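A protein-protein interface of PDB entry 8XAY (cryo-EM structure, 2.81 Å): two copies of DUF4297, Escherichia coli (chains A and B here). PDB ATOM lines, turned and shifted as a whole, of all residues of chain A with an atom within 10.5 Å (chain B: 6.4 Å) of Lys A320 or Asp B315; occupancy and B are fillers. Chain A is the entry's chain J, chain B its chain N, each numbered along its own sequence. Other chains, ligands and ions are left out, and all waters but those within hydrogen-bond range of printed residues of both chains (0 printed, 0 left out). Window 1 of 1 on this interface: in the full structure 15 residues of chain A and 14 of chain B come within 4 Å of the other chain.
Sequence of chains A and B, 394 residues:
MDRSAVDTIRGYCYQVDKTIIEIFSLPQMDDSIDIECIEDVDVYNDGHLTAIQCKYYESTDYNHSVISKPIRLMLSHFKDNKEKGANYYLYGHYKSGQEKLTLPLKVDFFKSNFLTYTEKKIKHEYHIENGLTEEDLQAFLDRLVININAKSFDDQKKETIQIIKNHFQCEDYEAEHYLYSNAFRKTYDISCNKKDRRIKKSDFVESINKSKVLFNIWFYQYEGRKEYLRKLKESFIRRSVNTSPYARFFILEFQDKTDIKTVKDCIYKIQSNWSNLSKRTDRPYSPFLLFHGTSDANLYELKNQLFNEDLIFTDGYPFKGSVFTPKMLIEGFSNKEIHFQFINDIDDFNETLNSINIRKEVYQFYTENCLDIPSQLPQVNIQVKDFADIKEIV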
ATOM      1  N   TYR A 300     -40.767  26.887 -25.580  1.00  0.00           N
ATOM      2  CA  TYR A 300     -39.498  27.104 -26.266  1.00  0.00           C
ATOM      3  C   TYR A 300     -39.701  27.389 -27.748  1.00  0.00           C
ATOM      4  O   TYR A 300     -38.867  28.062 -28.362  1.00  0.00           O
ATOM      5  CB  TYR A 300     -38.564  25.904 -26.081  1.00  0.00           C
ATOM      6  CG  TYR A 300     -38.142  25.615 -24.652  1.00  0.00           C
ATOM      7  CD1 TYR A 300     -38.177  26.602 -23.675  1.00  0.00           C
ATOM      8  CD2 TYR A 300     -37.694  24.352 -24.288  1.00  0.00           C
ATOM      9  CE1 TYR A 300     -37.786  26.335 -22.374  1.00  0.00           C
ATOM     10  CE2 TYR A 300     -37.302  24.077 -22.992  1.00  0.00           C
ATOM     11  CZ  TYR A 300     -37.350  25.071 -22.042  1.00  0.00           C
ATOM     12  OH  TYR A 300     -36.960  24.795 -20.753  1.00  0.00           O
ATOM     13  N   ASN A 304     -38.087  30.684 -29.825  1.00  0.00           N
ATOM     14  CA  ASN A 304     -37.193  30.602 -30.977  1.00  0.00           C
ATOM     15  C   ASN A 304     -37.655  31.489 -32.128  1.00  0.00           C
ATOM     16  O   ASN A 304     -36.830  32.155 -32.763  1.00  0.00           O
ATOM     17  CB  ASN A 304     -37.051  29.153 -31.441  1.00  0.00           C
ATOM     18  CG  ASN A 304     -36.202  28.325 -30.500  1.00  0.00           C
ATOM     19  OD1 ASN A 304     -35.037  28.057 -30.779  1.00  0.00           O
ATOM     20  ND2 ASN A 304     -36.776  27.925 -29.378  1.00  0.00           N
ATOM     21  N   ASP A 315     -33.337  35.656 -20.730  1.00  0.00           N
ATOM     22  CA  ASP A 315     -34.152  34.800 -19.880  1.00  0.00           C
ATOM     23  C   ASP A 315     -33.425  34.350 -18.619  1.00  0.00           C
ATOM     24  O   ASP A 315     -33.950  33.508 -17.885  1.00  0.00           O
ATOM     25  CB  ASP A 315     -34.646  33.582 -20.668  1.00  0.00           C
ATOM     26  CG  ASP A 315     -33.553  32.583 -20.950  1.00  0.00           C
ATOM     27  OD1 ASP A 315     -32.390  33.000 -21.135  1.00  0.00           O
ATOM     28  OD2 ASP A 315     -33.857  31.376 -20.999  1.00  0.00           O
ATOM     29  N   GLY A 316     -32.243  34.896 -18.342  1.00  0.00           N
ATOM     30  CA  GLY A 316     -31.469  34.505 -17.185  1.00  0.00           C
ATOM     31  C   GLY A 316     -30.555  33.319 -17.392  1.00  0.00           C
ATOM     32  O   GLY A 316     -29.837  32.944 -16.457  1.00  0.00           O
ATOM     33  N   TYR A 317     -30.554  32.715 -18.580  1.00  0.00           N
ATOM     34  CA  TYR A 317     -29.662  31.608 -18.920  1.00  0.00           C
ATOM     35  C   TYR A 317     -28.871  32.011 -20.155  1.00  0.00           C
ATOM     36  O   TYR A 317     -29.280  31.720 -21.290  1.00  0.00           O
ATOM     37  CB  TYR A 317     -30.425  30.304 -19.154  1.00  0.00           C
ATOM     38  CG  TYR A 317     -31.438  29.941 -18.087  1.00  0.00           C
ATOM     39  CD1 TYR A 317     -32.727  30.452 -18.108  1.00  0.00           C
ATOM     40  CD2 TYR A 317     -31.095  29.076 -17.059  1.00  0.00           C
ATOM     41  CE1 TYR A 317     -33.642  30.115 -17.132  1.00  0.00           C
ATOM     42  CE2 TYR A 317     -32.002  28.733 -16.082  1.00  0.00           C
ATOM     43  CZ  TYR A 317     -33.273  29.254 -16.122  1.00  0.00           C
ATOM     44  OH  TYR A 317     -34.177  28.910 -15.147  1.00  0.00           O
ATOM     45  N   PRO A 318     -27.730  32.686 -19.983  1.00  0.00           N
ATOM     46  CA  PRO A 318     -26.980  33.180 -21.148  1.00  0.00           C
ATOM     47  C   PRO A 318     -26.315  32.092 -21.971  1.00  0.00           C
ATOM     48  O   PRO A 318     -25.903  32.369 -23.104  1.00  0.00           O
ATOM     49  CB  PRO A 318     -25.941  34.116 -20.519  1.00  0.00           C
ATOM     50  CG  PRO A 318     -25.775  33.609 -19.133  1.00  0.00           C
ATOM     51  CD  PRO A 318     -27.111  33.090 -18.710  1.00  0.00           C
ATOM     52  N   PHE A 319     -26.187  30.875 -21.449  1.00  0.00           N
ATOM     53  CA  PHE A 319     -25.546  29.793 -22.178  1.00  0.00           C
ATOM     54  C   PHE A 319     -26.220  28.480 -21.807  1.00  0.00           C
ATOM     55  O   PHE A 319     -27.069  28.423 -20.916  1.00  0.00           O
ATOM     56  CB  PHE A 319     -24.034  29.746 -21.905  1.00  0.00           C
ATOM     57  CG  PHE A 319     -23.669  29.718 -20.448  1.00  0.00           C
ATOM     58  CD1 PHE A 319     -23.475  30.893 -19.746  1.00  0.00           C
ATOM     59  CD2 PHE A 319     -23.482  28.514 -19.792  1.00  0.00           C
ATOM     60  CE1 PHE A 319     -23.136  30.869 -18.414  1.00  0.00           C
ATOM     61  CE2 PHE A 319     -23.137  28.487 -18.461  1.00  0.00           C
ATOM     62  CZ  PHE A 319     -22.964  29.664 -17.771  1.00  0.00           C
ATOM     63  N   LYS A 320     -25.847  27.420 -22.518  1.00  0.00           N
ATOM     64  CA  LYS A 320     -26.436  26.112 -22.267  1.00  0.00           C
ATOM     65  C   LYS A 320     -25.888  25.533 -20.970  1.00  0.00           C
ATOM     66  O   LYS A 320     -24.682  25.592 -20.712  1.00  0.00           O
ATOM     67  CB  LYS A 320     -26.156  25.169 -23.435  1.00  0.00           C
ATOM     68  CG  LYS A 320     -26.825  23.811 -23.310  1.00  0.00           C
ATOM     69  CD  LYS A 320     -26.662  23.002 -24.580  1.00  0.00           C
ATOM     70  CE  LYS A 320     -27.995  22.466 -25.066  1.00  0.00           C
ATOM     71  NZ  LYS A 320     -27.871  21.816 -26.399  1.00  0.00           N
ATOM     72  N   GLY A 321     -26.775  24.977 -20.151  1.00  0.00           N
ATOM     73  CA  GLY A 321     -26.384  24.472 -18.853  1.00  0.00           C
ATOM     74  C   GLY A 321     -26.187  25.531 -17.797  1.00  0.00           C
ATOM     75  O   GLY A 321     -25.648  25.224 -16.728  1.00  0.00           O
ATOM     76  N   SER A 322     -26.601  26.765 -18.061  1.00  0.00           N
ATOM     77  CA  SER A 322     -26.421  27.844 -17.106  1.00  0.00           C
ATOM     78  C   SER A 322     -27.414  27.735 -15.958  1.00  0.00           C
ATOM     79  O   SER A 322     -28.561  27.319 -16.134  1.00  0.00           O
ATOM     80  CB  SER A 322     -26.589  29.199 -17.791  1.00  0.00           C
ATOM     81  OG  SER A 322     -26.613  30.249 -16.843  1.00  0.00           O
ATOM     82  N   VAL A 323     -26.953  28.113 -14.766  1.00  0.00           N
ATOM     83  CA  VAL A 323     -27.882  28.367 -13.679  1.00  0.00           C
ATOM     84  C   VAL A 323     -28.614  29.678 -13.945  1.00  0.00           C
ATOM     85  O   VAL A 323     -28.213  30.492 -14.785  1.00  0.00           O
ATOM     86  CB  VAL A 323     -27.159  28.398 -12.324  1.00  0.00           C
ATOM     87  CG1 VAL A 323     -26.578  27.034 -12.005  1.00  0.00           C
ATOM     88  CG2 VAL A 323     -26.076  29.461 -12.327  1.00  0.00           C
ATOM     89  N   PHE A 324     -29.708  29.881 -13.224  1.00  0.00           N
ATOM     90  CA  PHE A 324     -30.513  31.077 -13.431  1.00  0.00           C
ATOM     91  C   PHE A 324     -29.798  32.278 -12.825  1.00  0.00           C
ATOM     92  O   PHE A 324     -29.650  32.371 -11.602  1.00  0.00           O
ATOM     93  CB  PHE A 324     -31.896  30.908 -12.817  1.00  0.00           C
ATOM     94  CG  PHE A 324     -32.718  32.153 -12.860  1.00  0.00           C
ATOM     95  CD1 PHE A 324     -33.046  32.730 -14.070  1.00  0.00           C
ATOM     96  CD2 PHE A 324     -33.139  32.763 -11.694  1.00  0.00           C
ATOM     97  CE1 PHE A 324     -33.798  33.876 -14.117  1.00  0.00           C
ATOM     98  CE2 PHE A 324     -33.888  33.916 -11.737  1.00  0.00           C
ATOM     99  CZ  PHE A 324     -34.215  34.473 -12.948  1.00  0.00           C
ATOM    100  N   THR A 325     -29.351  33.195 -13.677  1.00  0.00           N
ATOM    101  CA  THR A 325     -28.681  34.405 -13.220  1.00  0.00           C
ATOM    102  C   THR A 325     -29.629  35.584 -13.371  1.00  0.00           C
ATOM    103  O   THR A 325     -29.886  36.021 -14.503  1.00  0.00           O
ATOM    104  CB  THR A 325     -27.398  34.648 -14.014  1.00  0.00           C
ATOM    105  OG1 THR A 325     -26.785  33.392 -14.326  1.00  0.00           O
ATOM    106  CG2 THR A 325     -26.427  35.486 -13.205  1.00  0.00           C
ATOM    107  N   TYR B 300     -20.574  22.022 -17.605  1.00  0.00           N
ATOM    108  CA  TYR B 300     -21.419  23.137 -17.200  1.00  0.00           C
ATOM    109  C   TYR B 300     -20.905  23.790 -15.926  1.00  0.00           C
ATOM    110  O   TYR B 300     -21.171  24.972 -15.688  1.00  0.00           O
ATOM    111  CB  TYR B 300     -22.863  22.674 -17.006  1.00  0.00           C
ATOM    112  CG  TYR B 300     -23.511  22.131 -18.258  1.00  0.00           C
ATOM    113  CD1 TYR B 300     -23.124  22.578 -19.514  1.00  0.00           C
ATOM    114  CD2 TYR B 300     -24.530  21.194 -18.182  1.00  0.00           C
ATOM    115  CE1 TYR B 300     -23.713  22.086 -20.657  1.00  0.00           C
ATOM    116  CE2 TYR B 300     -25.128  20.698 -19.320  1.00  0.00           C
ATOM    117  CZ  TYR B 300     -24.716  21.149 -20.555  1.00  0.00           C
ATOM    118  OH  TYR B 300     -25.310  20.661 -21.693  1.00  0.00           O
ATOM    119  N   LYS B 303     -18.301  26.163 -17.276  1.00  0.00           N
ATOM    120  CA  LYS B 303     -18.948  27.295 -17.930  1.00  0.00           C
ATOM    121  C   LYS B 303     -19.569  28.246 -16.915  1.00  0.00           C
ATOM    122  O   LYS B 303     -19.564  29.465 -17.116  1.00  0.00           O
ATOM    123  CB  LYS B 303     -20.012  26.796 -18.903  1.00  0.00           C
ATOM    124  CG  LYS B 303     -19.462  26.151 -20.147  1.00  0.00           C
ATOM    125  CD  LYS B 303     -20.544  25.395 -20.884  1.00  0.00           C
ATOM    126  CE  LYS B 303     -21.069  26.204 -22.046  1.00  0.00           C
ATOM    127  NZ  LYS B 303     -22.510  25.942 -22.286  1.00  0.00           N
ATOM    128  N   ASN B 304     -20.119  27.704 -15.826  1.00  0.00           N
ATOM    129  CA  ASN B 304     -20.752  28.548 -14.819  1.00  0.00           C
ATOM    130  C   ASN B 304     -19.722  29.358 -14.045  1.00  0.00           C
ATOM    131  O   ASN B 304     -19.983  30.508 -13.673  1.00  0.00           O
ATOM    132  CB  ASN B 304     -21.583  27.694 -13.866  1.00  0.00           C
ATOM    133  CG  ASN B 304     -22.956  27.390 -14.414  1.00  0.00           C
ATOM    134  OD1 ASN B 304     -23.770  28.290 -14.612  1.00  0.00           O
ATOM    135  ND2 ASN B 304     -23.223  26.117 -14.667  1.00  0.00           N
ATOM    136  N   PHE B 313     -18.729  34.688 -22.414  1.00  0.00           N
ATOM    137  CA  PHE B 313     -18.616  33.897 -23.628  1.00  0.00           C
ATOM    138  C   PHE B 313     -20.004  33.621 -24.191  1.00  0.00           C
ATOM    139  O   PHE B 313     -21.026  33.900 -23.558  1.00  0.00           O
ATOM    140  CB  PHE B 313     -17.874  32.574 -23.374  1.00  0.00           C
ATOM    141  CG  PHE B 313     -18.488  31.723 -22.293  1.00  0.00           C
ATOM    142  CD1 PHE B 313     -18.111  31.878 -20.972  1.00  0.00           C
ATOM    143  CD2 PHE B 313     -19.424  30.750 -22.605  1.00  0.00           C
ATOM    144  CE1 PHE B 313     -18.668  31.096 -19.984  1.00  0.00           C
ATOM    145  CE2 PHE B 313     -19.984  29.969 -21.620  1.00  0.00           C
ATOM    146  CZ  PHE B 313     -19.602  30.142 -20.309  1.00  0.00           C
ATOM    147  N   THR B 314     -20.026  33.070 -25.401  1.00  0.00           N
ATOM    148  CA  THR B 314     -21.242  32.586 -26.037  1.00  0.00           C
ATOM    149  C   THR B 314     -21.007  31.180 -26.563  1.00  0.00           C
ATOM    150  O   THR B 314     -19.920  30.867 -27.055  1.00  0.00           O
ATOM    151  CB  THR B 314     -21.688  33.489 -27.193  1.00  0.00           C
ATOM    152  OG1 THR B 314     -20.631  33.602 -28.151  1.00  0.00           O
ATOM    153  CG2 THR B 314     -22.083  34.864 -26.693  1.00  0.00           C
ATOM    154  N   ASP B 315     -22.028  30.332 -26.455  1.00  0.00           N
ATOM    155  CA  ASP B 315     -21.971  28.988 -27.014  1.00  0.00           C
ATOM    156  C   ASP B 315     -23.050  28.736 -28.058  1.00  0.00           C
ATOM    157  O   ASP B 315     -23.282  27.578 -28.425  1.00  0.00           O
ATOM    158  CB  ASP B 315     -22.061  27.934 -25.908  1.00  0.00           C
ATOM    159  CG  ASP B 315     -23.212  28.176 -24.964  1.00  0.00           C
ATOM    160  OD1 ASP B 315     -23.945  29.167 -25.150  1.00  0.00           O
ATOM    161  OD2 ASP B 315     -23.399  27.357 -24.043  1.00  0.00           O
ATOM    162  N   GLY B 316     -23.710  29.780 -28.549  1.00  0.00           N
ATOM    163  CA  GLY B 316     -24.771  29.603 -29.515  1.00  0.00           C
ATOM    164  C   GLY B 316     -26.121  29.271 -28.928  1.00  0.00           C
ATOM    165  O   GLY B 316     -27.044  28.945 -29.683  1.00  0.00           O
ATOM    166  N   TYR B 317     -26.273  29.348 -27.609  1.00  0.00           N
ATOM    167  CA  TYR B 317     -27.542  29.090 -26.934  1.00  0.00           C
ATOM    168  C   TYR B 317     -27.867  30.315 -26.094  1.00  0.00           C
ATOM    169  O   TYR B 317     -27.600  30.344 -24.885  1.00  0.00           O
ATOM    170  CB  TYR B 317     -27.475  27.824 -26.080  1.00  0.00           C
ATOM    171  CG  TYR B 317     -27.131  26.579 -26.864  1.00  0.00           C
ATOM    172  CD1 TYR B 317     -28.120  25.835 -27.488  1.00  0.00           C
ATOM    173  CD2 TYR B 317     -25.819  26.142 -26.967  1.00  0.00           C
ATOM    174  CE1 TYR B 317     -27.810  24.698 -28.204  1.00  0.00           C
ATOM    175  CE2 TYR B 317     -25.501  25.005 -27.680  1.00  0.00           C
ATOM    176  CZ  TYR B 317     -26.501  24.288 -28.296  1.00  0.00           C
ATOM    177  OH  TYR B 317     -26.189  23.154 -29.007  1.00  0.00           O
ATOM    178  N   PRO B 318     -28.441  31.356 -26.707  1.00  0.00           N
ATOM    179  CA  PRO B 318     -28.668  32.611 -25.971  1.00  0.00           C
ATOM    180  C   PRO B 318     -29.757  32.527 -24.915  1.00  0.00           C
ATOM    181  O   PRO B 318     -29.826  33.417 -24.059  1.00  0.00           O
ATOM    182  CB  PRO B 318     -29.044  33.601 -27.078  1.00  0.00           C
ATOM    183  CG  PRO B 318     -29.597  32.759 -28.166  1.00  0.00           C
ATOM    184  CD  PRO B 318     -28.893  31.438 -28.106  1.00  0.00           C
ATOM    185  N   PHE B 319     -30.604  31.502 -24.941  1.00  0.00           N
ATOM    186  CA  PHE B 319     -31.636  31.342 -23.929  1.00  0.00           C
ATOM    187  C   PHE B 319     -31.869  29.858 -23.692  1.00  0.00           C
ATOM    188  O   PHE B 319     -31.337  29.002 -24.401  1.00  0.00           O
ATOM    189  CB  PHE B 319     -32.939  32.063 -24.316  1.00  0.00           C
ATOM    190  CG  PHE B 319     -33.437  31.748 -25.699  1.00  0.00           C
ATOM    191  CD1 PHE B 319     -33.025  32.496 -26.788  1.00  0.00           C
ATOM    192  CD2 PHE B 319     -34.332  30.714 -25.908  1.00  0.00           C
ATOM    193  CE1 PHE B 319     -33.485  32.212 -28.053  1.00  0.00           C
ATOM    194  CE2 PHE B 319     -34.793  30.426 -27.171  1.00  0.00           C
ATOM    195  CZ  PHE B 319     -34.370  31.175 -28.245  1.00  0.00           C
ATOM    196  N   SER B 322     -32.989  26.839 -26.402  1.00  0.00           N
ATOM    197  CA  SER B 322     -32.703  27.392 -27.713  1.00  0.00           C
ATOM    198  C   SER B 322     -32.049  26.355 -28.613  1.00  0.00           C
ATOM    199  O   SER B 322     -31.286  25.497 -28.163  1.00  0.00           O
ATOM    200  CB  SER B 322     -31.784  28.607 -27.596  1.00  0.00           C
ATOM    201  OG  SER B 322     -31.278  28.985 -28.862  1.00  0.00           O
ATOM    202  N   PHE B 324     -29.257  25.721 -31.617  1.00  0.00           N
ATOM    203  CA  PHE B 324     -27.913  26.265 -31.753  1.00  0.00           C
ATOM    204  C   PHE B 324     -27.902  27.387 -32.781  1.00  0.00           C
ATOM    205  O   PHE B 324     -28.291  27.188 -33.935  1.00  0.00           O
ATOM    206  CB  PHE B 324     -26.929  25.171 -32.143  1.00  0.00           C
ATOM    207  CG  PHE B 324     -25.538  25.673 -32.373  1.00  0.00           C
ATOM    208  CD1 PHE B 324     -24.879  26.386 -31.387  1.00  0.00           C
ATOM    209  CD2 PHE B 324     -24.880  25.417 -33.561  1.00  0.00           C
ATOM    210  CE1 PHE B 324     -23.596  26.840 -31.588  1.00  0.00           C
ATOM    211  CE2 PHE B 324     -23.597  25.873 -33.768  1.00  0.00           C
ATOM    212  CZ  PHE B 324     -22.954  26.587 -32.779  1.00  0.00           C
ATOM    213  N   THR B 325     -27.455  28.565 -32.356  1.00  0.00           N
ATOM    214  CA  THR B 325     -27.380  29.732 -33.225  1.00  0.00           C
ATOM    215  C   THR B 325     -25.920  30.075 -33.473  1.00  0.00           C
ATOM    216  O   THR B 325     -25.277  30.699 -32.615  1.00  0.00           O
ATOM    217  CB  THR B 325     -28.111  30.922 -32.597  1.00  0.00           C
ATOM    218  OG1 THR B 325     -29.428  30.522 -32.204  1.00  0.00           O
ATOM    219  CG2 THR B 325     -28.212  32.066 -33.589  1.00  0.00           C
ATOM    220  N   MET B 328     -24.670  33.860 -33.165  1.00  0.00           N
ATOM    221  CA  MET B 328     -24.198  34.407 -31.898  1.00  0.00           C
ATOM    222  C   MET B 328     -22.680  34.328 -31.791  1.00  0.00           C
ATOM    223  O   MET B 328     -22.043  35.224 -31.227  1.00  0.00           O
ATOM    224  CB  MET B 328     -24.857  33.673 -30.731  1.00  0.00           C
ATOM    225  CG  MET B 328     -26.345  33.939 -30.595  1.00  0.00           C
ATOM    226  SD  MET B 328     -26.754  35.682 -30.778  1.00  0.00           S
ATOM    227  CE  MET B 328     -26.702  36.220 -29.073  1.00  0.00           C
ATOM    228  N   LEU B 329     -22.084  33.257 -32.316  1.00  0.00           N
ATOM    229  CA  LEU B 329     -20.632  33.157 -32.371  1.00  0.00           C
ATOM    230  C   LEU B 329     -20.025  34.011 -33.476  1.00  0.00           C
ATOM    231  O   LEU B 329     -18.837  34.339 -33.398  1.00  0.00           O
ATOM    232  CB  LEU B 329     -20.206  31.700 -32.548  1.00  0.00           C
ATOM    233  CG  LEU B 329     -20.596  30.745 -31.419  1.00  0.00           C
ATOM    234  CD1 LEU B 329     -21.776  29.907 -31.835  1.00  0.00           C
ATOM    235  CD2 LEU B 329     -19.432  29.855 -31.042  1.00  0.00           C
ATOM    236  N   GLN B 341     -15.343  32.210 -27.237  1.00  0.00           N
ATOM    237  CA  GLN B 341     -16.512  31.453 -27.655  1.00  0.00           C
ATOM    238  C   GLN B 341     -16.386  30.018 -27.175  1.00  0.00           C
ATOM    239  O   GLN B 341     -15.311  29.420 -27.251  1.00  0.00           O
ATOM    240  CB  GLN B 341     -16.673  31.476 -29.171  1.00  0.00           C
ATOM    241  CG  GLN B 341     -17.092  32.817 -29.726  1.00  0.00           C
ATOM    242  CD  GLN B 341     -15.910  33.696 -30.055  1.00  0.00           C
ATOM    243  OE1 GLN B 341     -15.881  34.868 -29.699  1.00  0.00           O
ATOM    244  NE2 GLN B 341     -14.926  33.132 -30.736  1.00  0.00           N
ATOM    245  N   PHE B 342     -17.491  29.471 -26.689  1.00  0.00           N
ATOM    246  CA  PHE B 342     -17.545  28.102 -26.201  1.00  0.00           C
ATOM    247  C   PHE B 342     -18.228  27.219 -27.233  1.00  0.00           C
ATOM    248  O   PHE B 342     -19.184  27.639 -27.887  1.00  0.00           O
ATOM    249  CB  PHE B 342     -18.294  28.027 -24.870  1.00  0.00           C
ATOM    250  CG  PHE B 342     -17.644  27.132 -23.859  1.00  0.00           C
ATOM    251  CD1 PHE B 342     -17.815  25.760 -23.920  1.00  0.00           C
ATOM    252  CD2 PHE B 342     -16.863  27.662 -22.848  1.00  0.00           C
ATOM    253  CE1 PHE B 342     -17.219  24.935 -22.989  1.00  0.00           C
ATOM    254  CE2 PHE B 342     -16.263  26.843 -21.916  1.00  0.00           C
ATOM    255  CZ  PHE B 342     -16.441  25.477 -21.987  1.00  0.00           C
ATOM    256  N   ILE B 343     -17.716  26.005 -27.401  1.00  0.00           N
ATOM    257  CA  ILE B 343     -18.342  24.998 -28.247  1.00  0.00           C
ATOM    258  C   ILE B 343     -18.568  23.757 -27.397  1.00  0.00           C
ATOM    259  O   ILE B 343     -17.654  23.303 -26.699  1.00  0.00           O
ATOM    260  CB  ILE B 343     -17.492  24.677 -29.490  1.00  0.00           C
ATOM    261  CG1 ILE B 343     -17.160  25.958 -30.259  1.00  0.00           C
ATOM    262  CG2 ILE B 343     -18.234  23.717 -30.390  1.00  0.00           C
ATOM    263  CD1 ILE B 343     -16.473  25.729 -31.582  1.00  0.00           C
ATOM    264  N   ASN B 344     -19.787  23.220 -27.446  1.00  0.00           N
ATOM    265  CA  ASN B 344     -20.169  22.155 -26.526  1.00  0.00           C
ATOM    266  C   ASN B 344     -19.616  20.803 -26.963  1.00  0.00           C
ATOM    267  O   ASN B 344     -18.918  20.131 -26.196  1.00  0.00           O
ATOM    268  CB  ASN B 344     -21.692  22.106 -26.399  1.00  0.00           C
ATOM    269  CG  ASN B 344     -22.237  23.229 -25.545  1.00  0.00           C
ATOM    270  OD1 ASN B 344     -22.493  23.053 -24.355  1.00  0.00           O
ATOM    271  ND2 ASN B 344     -22.409  24.398 -26.148  1.00  0.00           N
ATOM    272  N   ASP B 348     -21.875  20.866 -32.612  1.00  0.00           N
ATOM    273  CA  ASP B 348     -21.841  22.320 -32.560  1.00  0.00           C
ATOM    274  C   ASP B 348     -20.609  22.863 -33.270  1.00  0.00           C
ATOM    275  O   ASP B 348     -20.638  23.976 -33.804  1.00  0.00           O
ATOM    276  CB  ASP B 348     -21.861  22.781 -31.104  1.00  0.00           C
ATOM    277  CG  ASP B 348     -23.234  22.661 -30.478  1.00  0.00           C
ATOM    278  OD1 ASP B 348     -24.128  23.440 -30.841  1.00  0.00           O
ATOM    279  OD2 ASP B 348     -23.423  21.785 -29.612  1.00  0.00           O
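NZ of Lys A320 sits at hydrogen-bond distance from OH of Tyr B317 (3.4 Å).
The backbone carbonyl oxygen of Gly A321 lies within hydrogen-bond range of the side-chain amide nitrogen of Asn B304.
O of Lys A320 is in hydrogen-bond range of NZ of Lys B303, at 2.7 Å.
N of Val A323 is in hydrogen-bond range of OD1 of Asn B304 (3.2 Å).
O of Pro A318 lies close to O of Tyr B317 (3.2 Å).
The backbone carbonyl oxygen (O) of Pro B318 lies close to the backbone carbonyl oxygen (O) of Tyr A317 (3.3 Å).
N of Lys A320 lies within hydrogen-bond range of OD2 of Asp B315 (2.9 Å).
The side-chain hydroxyl (OH) of Tyr B317 lies within hydrogen-bond range of the side-chain carboxylate (OD1) of Asp B348, 2.8 Å away.
The side-chain carboxylate (OD1) of Asp B315 lies close to the backbone NH (N) of Tyr B317, at 3.4 Å.
NZ of Lys B303 is in salt-bridge range of OD2 of Asp B315 (2.4 Å).
OD1 of Asp A315 lies within hydrogen-bond range of N of Tyr A317.
O of Val A323 is in hydrogen-bond range of OG1 of Thr A325 (3.3 Å).
The backbone carbonyl oxygen (O) of Tyr B300 is in hydrogen-bond range of the side-chain amide nitrogen (ND2) of Asn B304 (2.6 Å).
Asn A304 touches Phe B319 (ND2 to CE2, 3.9 Å).
Asn A304 touches Ser B322.
CA of Phe B319 touches O of Tyr A317, 3.6 Å away.
O of Pro A318 touches CA of Pro B318 (3.99 Å).
Lys B303 touches Phe A319.
Asn B304 touches Phe A319.
CG of Phe A319 touches CE2 of Phe B313, at 3.9 Å.
Phe A319 touches Asp B315 (CB to OD2, 3.3 Å).
CD1 of Tyr B300 touches O of Lys A320, 3.6 Å away.
Asn B304 touches Ser A322 (OD1 to CA, 3.7 Å).
Lys A320 touches four residues of chain B.
Tyr B300 touches just these residues of chain A: Lys A320 and Gly A321.
No residue of chain A comes within 4 Å of Gly B316.
Printed residues of chain A within 4 Å of Pro B318: Asp A315, Tyr A317 and Pro A318.
Of the printed residues of chain A, Phe B313 touches Phe A319.
Of the printed residues of chain B, Gly A321 touches Tyr B300 (3.8 Å) and Asn B304 (3.3 Å).
Gly A316 touches none of the printed residues of chain B.
Phe B324 touches none of the printed residues of chain A.
The nearest residue of chain B that does not touch Lys A320 is Asn B344 (4.2 Å).
The nearest residue of chain A that does not touch Asp B315 is Pro A318 (4.3 Å).
The nearest printed residue of chain A that does not touch Phe B319 is Tyr A300 (4.9 Å).
Of the 13 printed residues of chain A, 9 touch a printed residue of chain B.
Hydrophobic or aromatic side chains of chain B within 4 Å of the printed part of chain A: Tyr B300, Phe B313, Tyr B317 and Phe B319.
Along chain B the printed residues that touch a printed residue of chain A span positions 300 to 322.
Among the printed residues, 21 pairs touch across the chains.
Among the printed residues, no Asp or Glu carboxylate lies within 4 Å of a Lys or Arg side-chain nitrogen of the other chain.
Asn A304 touches Phe B319, and with the chains exchanged Phe A319 touches Asn B304.
Asn A304 touches Ser B322, and with the chains exchanged Ser A322 touches Asn B304.
Asp A315 touches Phe B319, and with the chains exchanged Phe A319 touches Asp B315.
Tyr A317 touches Phe B319, and with the chains exchanged Phe A319 touches Tyr B317.
10 positions are printed for both chains.
Of the 21 pairs that touch across the chains among the printed residues, 11 have their exchanged pair printed and touching as well.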
